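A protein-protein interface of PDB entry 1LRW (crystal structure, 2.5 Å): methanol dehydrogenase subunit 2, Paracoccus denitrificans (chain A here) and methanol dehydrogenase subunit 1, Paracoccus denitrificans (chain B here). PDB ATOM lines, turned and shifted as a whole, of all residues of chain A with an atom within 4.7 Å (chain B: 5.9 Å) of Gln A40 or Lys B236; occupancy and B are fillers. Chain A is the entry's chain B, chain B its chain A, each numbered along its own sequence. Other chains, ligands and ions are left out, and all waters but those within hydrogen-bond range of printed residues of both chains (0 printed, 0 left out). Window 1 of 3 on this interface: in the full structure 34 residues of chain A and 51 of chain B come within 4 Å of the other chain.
The side-chain amide nitrogen of Gln A40 sits at hydrogen-bond distance from the backbone carbonyl oxygen of Gly B179 (2.9 Å).
The backbone NH (N) of Arg B181 lies within hydrogen-bond range of the side-chain amide oxygen (OE1) of Gln A40.
The side-chain hydroxyl of Tyr B425 is in hydrogen-bond range of the side-chain amide nitrogen of Gln A40 (3.5 Å).
O of Lys B236 lies within hydrogen-bond range of NE2 of Gln A40 (3.4 Å).
O of Thr B201 sits at hydrogen-bond distance from NH1 of Arg B181, at 2.5 Å.
Leu A37 touches Asp B233 (CD1 to CB, 3.7 Å).
Leu A37 touches Lys B236 (O to CD, 3.9 Å).
Ile B237 touches Leu A37.
Tyr B425 touches Leu A37 (CD2 to CD2, 3.997 Å).
CG of Lys A39 touches CB of Ala B427 (3.5 Å).
Gln A40 touches Val B180 (OE1 to CA, 3.6 Å).
NE2 of Gln A40 touches CG2 of Ile B237 (3.5 Å).
Ser A38 touches none of the printed residues of chain B.
Of the printed residues of chain B, Lys A39 touches Ala B427 (3.5 Å).
Gln A40 touches just these residues of chain B: Gly B179, Val B180, Arg B181, Lys B236, Ile B237 and Tyr B425.
Gly A41 touches none of the printed residues of chain B.
Printed residues of chain A within 4 Å of Asp B233: Leu A37 (3.7 Å).
Lys B236 touches two residues of chain A.
Of the printed residues of chain A, Tyr B425 touches Leu A37 and Gln A40.
Hydrophobic or aromatic side chains of chain B within 4 Å of the printed part of chain A: Val B180, Ile B237, Tyr B425 and Ala B427.
Along chain B the printed residues that touch a printed residue of chain A span positions 179 to 427.
Of the 8 printed residues of chain A, 3 touch a printed residue of chain B.
Hydrophobic or aromatic side chains of chain A that line the printed part of chain B: Leu A37.
Along chain A the printed residues that touch a printed residue of chain B span positions 37 to 40.
Among the printed residues, no Asp or Glu carboxylate lies within 4 Å of a Lys or Arg side-chain nitrogen of the other chain.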
ATOM      1  N   LEU A  37      23.844  32.096 -25.656  1.00  0.00           N
ATOM      2  CA  LEU A  37      22.568  31.818 -26.299  1.00  0.00           C
ATOM      3  C   LEU A  37      22.708  31.342 -27.739  1.00  0.00           C
ATOM      4  O   LEU A  37      21.758  30.823 -28.322  1.00  0.00           O
ATOM      5  CB  LEU A  37      21.670  33.061 -26.261  1.00  0.00           C
ATOM      6  CG  LEU A  37      21.409  33.752 -24.912  1.00  0.00           C
ATOM      7  CD1 LEU A  37      20.331  34.805 -25.120  1.00  0.00           C
ATOM      8  CD2 LEU A  37      20.971  32.755 -23.836  1.00  0.00           C
ATOM      9  N   SER A  38      23.893  31.501 -28.312  1.00  0.00           N
ATOM     10  CA  SER A  38      24.122  31.109 -29.698  1.00  0.00           C
ATOM     11  C   SER A  38      24.719  29.725 -29.920  1.00  0.00           C
ATOM     12  O   SER A  38      24.664  29.208 -31.032  1.00  0.00           O
ATOM     13  CB  SER A  38      25.015  32.145 -30.383  1.00  0.00           C
ATOM     14  OG  SER A  38      24.373  33.405 -30.440  1.00  0.00           O
ATOM     15  N   LYS A  39      25.287  29.127 -28.877  1.00  0.00           N
ATOM     16  CA  LYS A  39      25.910  27.810 -28.998  1.00  0.00           C
ATOM     17  C   LYS A  39      25.034  26.768 -29.697  1.00  0.00           C
ATOM     18  O   LYS A  39      25.499  26.063 -30.595  1.00  0.00           O
ATOM     19  CB  LYS A  39      26.296  27.281 -27.619  1.00  0.00           C
ATOM     20  CG  LYS A  39      27.186  28.195 -26.798  1.00  0.00           C
ATOM     21  CD  LYS A  39      28.582  28.296 -27.362  1.00  0.00           C
ATOM     22  CE  LYS A  39      29.505  29.042 -26.394  1.00  0.00           C
ATOM     23  NZ  LYS A  39      29.759  28.290 -25.129  1.00  0.00           N
ATOM     24  N   GLN A  40      23.774  26.665 -29.282  1.00  0.00           N
ATOM     25  CA  GLN A  40      22.846  25.698 -29.864  1.00  0.00           C
ATOM     26  C   GLN A  40      22.689  25.812 -31.371  1.00  0.00           C
ATOM     27  O   GLN A  40      22.858  24.830 -32.091  1.00  0.00           O
ATOM     28  CB  GLN A  40      21.461  25.845 -29.246  1.00  0.00           C
ATOM     29  CG  GLN A  40      21.321  25.310 -27.852  1.00  0.00           C
ATOM     30  CD  GLN A  40      19.901  25.431 -27.351  1.00  0.00           C
ATOM     31  OE1 GLN A  40      18.962  24.936 -27.984  1.00  0.00           O
ATOM     32  NE2 GLN A  40      19.730  26.088 -26.209  1.00  0.00           N
ATOM     33  N   GLY A  41      22.330  27.005 -31.831  1.00  0.00           N
ATOM     34  CA  GLY A  41      22.123  27.233 -33.246  1.00  0.00           C
ATOM     35  C   GLY A  41      23.367  26.923 -34.042  1.00  0.00           C
ATOM     36  O   GLY A  41      23.296  26.311 -35.112  1.00  0.00           O
ATOM     37  N   GLU A  42      24.513  27.349 -33.520  1.00  0.00           N
ATOM     38  CA  GLU A  42      25.786  27.102 -34.187  1.00  0.00           C
ATOM     39  C   GLU A  42      25.971  25.597 -34.343  1.00  0.00           C
ATOM     40  O   GLU A  42      26.361  25.111 -35.401  1.00  0.00           O
ATOM     41  CB  GLU A  42      26.943  27.684 -33.363  1.00  0.00           C
ATOM     42  CG  GLU A  42      26.939  29.205 -33.244  1.00  0.00           C
ATOM     43  CD  GLU A  42      28.030  29.731 -32.314  1.00  0.00           C
ATOM     44  OE1 GLU A  42      28.192  30.971 -32.218  1.00  0.00           O
ATOM     45  OE2 GLU A  42      28.722  28.906 -31.675  1.00  0.00           O
ATOM     46  N   SER A  43      25.674  24.871 -33.274  1.00  0.00           N
ATOM     47  CA  SER A  43      25.802  23.424 -33.252  1.00  0.00           C
ATOM     48  C   SER A  43      24.956  22.737 -34.327  1.00  0.00           C
ATOM     49  O   SER A  43      25.448  21.874 -35.049  1.00  0.00           O
ATOM     50  CB  SER A  43      25.414  22.898 -31.869  1.00  0.00           C
ATOM     51  OG  SER A  43      25.670  21.508 -31.774  1.00  0.00           O
ATOM     52  N   LEU A  44      23.685  23.109 -34.427  1.00  0.00           N
ATOM     53  CA  LEU A  44      22.821  22.511 -35.433  1.00  0.00           C
ATOM     54  C   LEU A  44      23.398  22.776 -36.812  1.00  0.00           C
ATOM     55  O   LEU A  44      23.315  21.938 -37.705  1.00  0.00           O
ATOM     56  CB  LEU A  44      21.419  23.106 -35.369  1.00  0.00           C
ATOM     57  CG  LEU A  44      20.491  22.699 -34.231  1.00  0.00           C
ATOM     58  CD1 LEU A  44      19.151  23.396 -34.419  1.00  0.00           C
ATOM     59  CD2 LEU A  44      20.309  21.189 -34.226  1.00  0.00           C
ATOM     60  N   VAL B 154      25.827  20.543 -25.845  1.00  0.00           N
ATOM     61  CA  VAL B 154      24.939  21.599 -25.366  1.00  0.00           C
ATOM     62  C   VAL B 154      23.837  21.009 -24.495  1.00  0.00           C
ATOM     63  O   VAL B 154      22.823  21.649 -24.262  1.00  0.00           O
ATOM     64  CB  VAL B 154      24.266  22.362 -26.528  1.00  0.00           C
ATOM     65  CG1 VAL B 154      25.310  22.917 -27.464  1.00  0.00           C
ATOM     66  CG2 VAL B 154      23.328  21.444 -27.272  1.00  0.00           C
ATOM     67  N   LEU B 178      18.411  21.511 -19.585  1.00  0.00           N
ATOM     68  CA  LEU B 178      19.730  22.002 -19.965  1.00  0.00           C
ATOM     69  C   LEU B 178      19.547  23.246 -20.850  1.00  0.00           C
ATOM     70  O   LEU B 178      20.504  23.758 -21.436  1.00  0.00           O
ATOM     71  CB  LEU B 178      20.491  20.917 -20.746  1.00  0.00           C
ATOM     72  CG  LEU B 178      20.948  19.581 -20.134  1.00  0.00           C
ATOM     73  CD1 LEU B 178      22.284  19.763 -19.454  1.00  0.00           C
ATOM     74  CD2 LEU B 178      19.905  19.039 -19.177  1.00  0.00           C
ATOM     75  N   GLY B 179      18.309  23.718 -20.955  1.00  0.00           N
ATOM     76  CA  GLY B 179      18.028  24.894 -21.757  1.00  0.00           C
ATOM     77  C   GLY B 179      17.949  24.670 -23.255  1.00  0.00           C
ATOM     78  O   GLY B 179      17.927  25.623 -24.024  1.00  0.00           O
ATOM     79  N   VAL B 180      17.909  23.421 -23.691  1.00  0.00           N
ATOM     80  CA  VAL B 180      17.828  23.146 -25.121  1.00  0.00           C
ATOM     81  C   VAL B 180      16.483  23.557 -25.711  1.00  0.00           C
ATOM     82  O   VAL B 180      15.436  23.185 -25.190  1.00  0.00           O
ATOM     83  CB  VAL B 180      18.033  21.653 -25.414  1.00  0.00           C
ATOM     84  CG1 VAL B 180      17.727  21.366 -26.864  1.00  0.00           C
ATOM     85  CG2 VAL B 180      19.451  21.251 -25.089  1.00  0.00           C
ATOM     86  N   ARG B 181      16.522  24.326 -26.798  1.00  0.00           N
ATOM     87  CA  ARG B 181      15.315  24.766 -27.497  1.00  0.00           C
ATOM     88  C   ARG B 181      14.810  23.554 -28.279  1.00  0.00           C
ATOM     89  O   ARG B 181      15.535  23.009 -29.108  1.00  0.00           O
ATOM     90  CB  ARG B 181      15.658  25.901 -28.461  1.00  0.00           C
ATOM     91  CG  ARG B 181      14.492  26.415 -29.292  1.00  0.00           C
ATOM     92  CD  ARG B 181      14.994  27.400 -30.325  1.00  0.00           C
ATOM     93  NE  ARG B 181      13.981  27.717 -31.324  1.00  0.00           N
ATOM     94  CZ  ARG B 181      14.249  28.252 -32.511  1.00  0.00           C
ATOM     95  NH1 ARG B 181      13.268  28.511 -33.364  1.00  0.00           N
ATOM     96  NH2 ARG B 181      15.503  28.512 -32.850  1.00  0.00           N
ATOM     97  N   GLY B 182      13.571  23.147 -28.016  1.00  0.00           N
ATOM     98  CA  GLY B 182      13.006  21.972 -28.660  1.00  0.00           C
ATOM     99  C   GLY B 182      12.723  22.016 -30.145  1.00  0.00           C
ATOM    100  O   GLY B 182      12.383  23.061 -30.700  1.00  0.00           O
ATOM    101  N   THR B 201       9.775  27.316 -30.476  1.00  0.00           N
ATOM    102  CA  THR B 201       9.833  28.717 -30.061  1.00  0.00           C
ATOM    103  C   THR B 201      10.584  29.564 -31.087  1.00  0.00           C
ATOM    104  O   THR B 201      11.334  29.036 -31.898  1.00  0.00           O
ATOM    105  CB  THR B 201      10.543  28.877 -28.686  1.00  0.00           C
ATOM    106  OG1 THR B 201      11.936  28.555 -28.816  1.00  0.00           O
ATOM    107  CG2 THR B 201       9.905  27.968 -27.643  1.00  0.00           C
ATOM    108  N   ASP B 233      15.658  37.559 -26.069  1.00  0.00           N
ATOM    109  CA  ASP B 233      16.138  36.333 -26.707  1.00  0.00           C
ATOM    110  C   ASP B 233      15.962  35.079 -25.855  1.00  0.00           C
ATOM    111  O   ASP B 233      16.474  34.015 -26.206  1.00  0.00           O
ATOM    112  CB  ASP B 233      17.625  36.468 -27.044  1.00  0.00           C
ATOM    113  CG  ASP B 233      17.872  37.217 -28.333  1.00  0.00           C
ATOM    114  OD1 ASP B 233      19.057  37.468 -28.638  1.00  0.00           O
ATOM    115  OD2 ASP B 233      16.896  37.546 -29.042  1.00  0.00           O
ATOM    116  N   ALA B 234      15.244  35.203 -24.746  1.00  0.00           N
ATOM    117  CA  ALA B 234      15.040  34.077 -23.842  1.00  0.00           C
ATOM    118  C   ALA B 234      14.555  32.812 -24.535  1.00  0.00           C
ATOM    119  O   ALA B 234      14.817  31.703 -24.063  1.00  0.00           O
ATOM    120  CB  ALA B 234      14.073  34.470 -22.732  1.00  0.00           C
ATOM    121  N   TRP B 235      13.863  32.973 -25.660  1.00  0.00           N
ATOM    122  CA  TRP B 235      13.342  31.824 -26.397  1.00  0.00           C
ATOM    123  C   TRP B 235      14.425  30.969 -27.068  1.00  0.00           C
ATOM    124  O   TRP B 235      14.159  29.849 -27.505  1.00  0.00           O
ATOM    125  CB  TRP B 235      12.336  32.290 -27.447  1.00  0.00           C
ATOM    126  CG  TRP B 235      12.908  33.272 -28.401  1.00  0.00           C
ATOM    127  CD1 TRP B 235      12.924  34.627 -28.268  1.00  0.00           C
ATOM    128  CD2 TRP B 235      13.622  32.975 -29.606  1.00  0.00           C
ATOM    129  NE1 TRP B 235      13.608  35.198 -29.316  1.00  0.00           N
ATOM    130  CE2 TRP B 235      14.049  34.206 -30.152  1.00  0.00           C
ATOM    131  CE3 TRP B 235      13.947  31.788 -30.276  1.00  0.00           C
ATOM    132  CZ2 TRP B 235      14.785  34.286 -31.337  1.00  0.00           C
ATOM    133  CZ3 TRP B 235      14.681  31.866 -31.459  1.00  0.00           C
ATOM    134  CH2 TRP B 235      15.092  33.106 -31.975  1.00  0.00           C
ATOM    135  N   LYS B 236      15.641  31.492 -27.157  1.00  0.00           N
ATOM    136  CA  LYS B 236      16.721  30.738 -27.780  1.00  0.00           C
ATOM    137  C   LYS B 236      17.072  29.547 -26.907  1.00  0.00           C
ATOM    138  O   LYS B 236      17.633  28.559 -27.383  1.00  0.00           O
ATOM    139  CB  LYS B 236      17.962  31.613 -27.982  1.00  0.00           C
ATOM    140  CG  LYS B 236      17.720  32.810 -28.866  1.00  0.00           C
ATOM    141  CD  LYS B 236      18.977  33.191 -29.636  1.00  0.00           C
ATOM    142  CE  LYS B 236      18.735  34.432 -30.482  1.00  0.00           C
ATOM    143  NZ  LYS B 236      19.675  34.517 -31.631  1.00  0.00           N
ATOM    144  N   ILE B 237      16.727  29.646 -25.629  1.00  0.00           N
ATOM    145  CA  ILE B 237      17.002  28.584 -24.667  1.00  0.00           C
ATOM    146  C   ILE B 237      15.728  28.222 -23.907  1.00  0.00           C
ATOM    147  O   ILE B 237      15.788  27.841 -22.742  1.00  0.00           O
ATOM    148  CB  ILE B 237      18.078  29.032 -23.626  1.00  0.00           C
ATOM    149  CG1 ILE B 237      17.745  30.437 -23.112  1.00  0.00           C
ATOM    150  CG2 ILE B 237      19.472  29.000 -24.241  1.00  0.00           C
ATOM    151  CD1 ILE B 237      18.646  30.913 -22.001  1.00  0.00           C
ATOM    152  N   GLY B 238      14.580  28.319 -24.573  1.00  0.00           N
ATOM    153  CA  GLY B 238      13.317  28.045 -23.904  1.00  0.00           C
ATOM    154  C   GLY B 238      12.666  26.675 -24.001  1.00  0.00           C
ATOM    155  O   GLY B 238      11.437  26.584 -24.093  1.00  0.00           O
ATOM    156  N   TYR B 425      23.073  30.770 -17.513  1.00  0.00           N
ATOM    157  CA  TYR B 425      22.953  29.748 -18.529  1.00  0.00           C
ATOM    158  C   TYR B 425      24.306  29.507 -19.179  1.00  0.00           C
ATOM    159  O   TYR B 425      24.884  30.425 -19.754  1.00  0.00           O
ATOM    160  CB  TYR B 425      21.953  30.166 -19.607  1.00  0.00           C
ATOM    161  CG  TYR B 425      22.000  29.255 -20.806  1.00  0.00           C
ATOM    162  CD1 TYR B 425      21.472  27.972 -20.743  1.00  0.00           C
ATOM    163  CD2 TYR B 425      22.656  29.644 -21.976  1.00  0.00           C
ATOM    164  CE1 TYR B 425      21.600  27.091 -21.807  1.00  0.00           C
ATOM    165  CE2 TYR B 425      22.790  28.772 -23.049  1.00  0.00           C
ATOM    166  CZ  TYR B 425      22.259  27.493 -22.958  1.00  0.00           C
ATOM    167  OH  TYR B 425      22.374  26.615 -24.015  1.00  0.00           O
ATOM    168  N   ALA B 427      25.937  26.813 -21.853  1.00  0.00           N
ATOM    169  CA  ALA B 427      25.709  25.686 -22.752  1.00  0.00           C
ATOM    170  C   ALA B 427      26.426  24.421 -22.283  1.00  0.00           C
ATOM    171  O   ALA B 427      27.647  24.406 -22.125  1.00  0.00           O
ATOM    172  CB  ALA B 427      26.145  26.044 -24.173  1.00  0.00           C
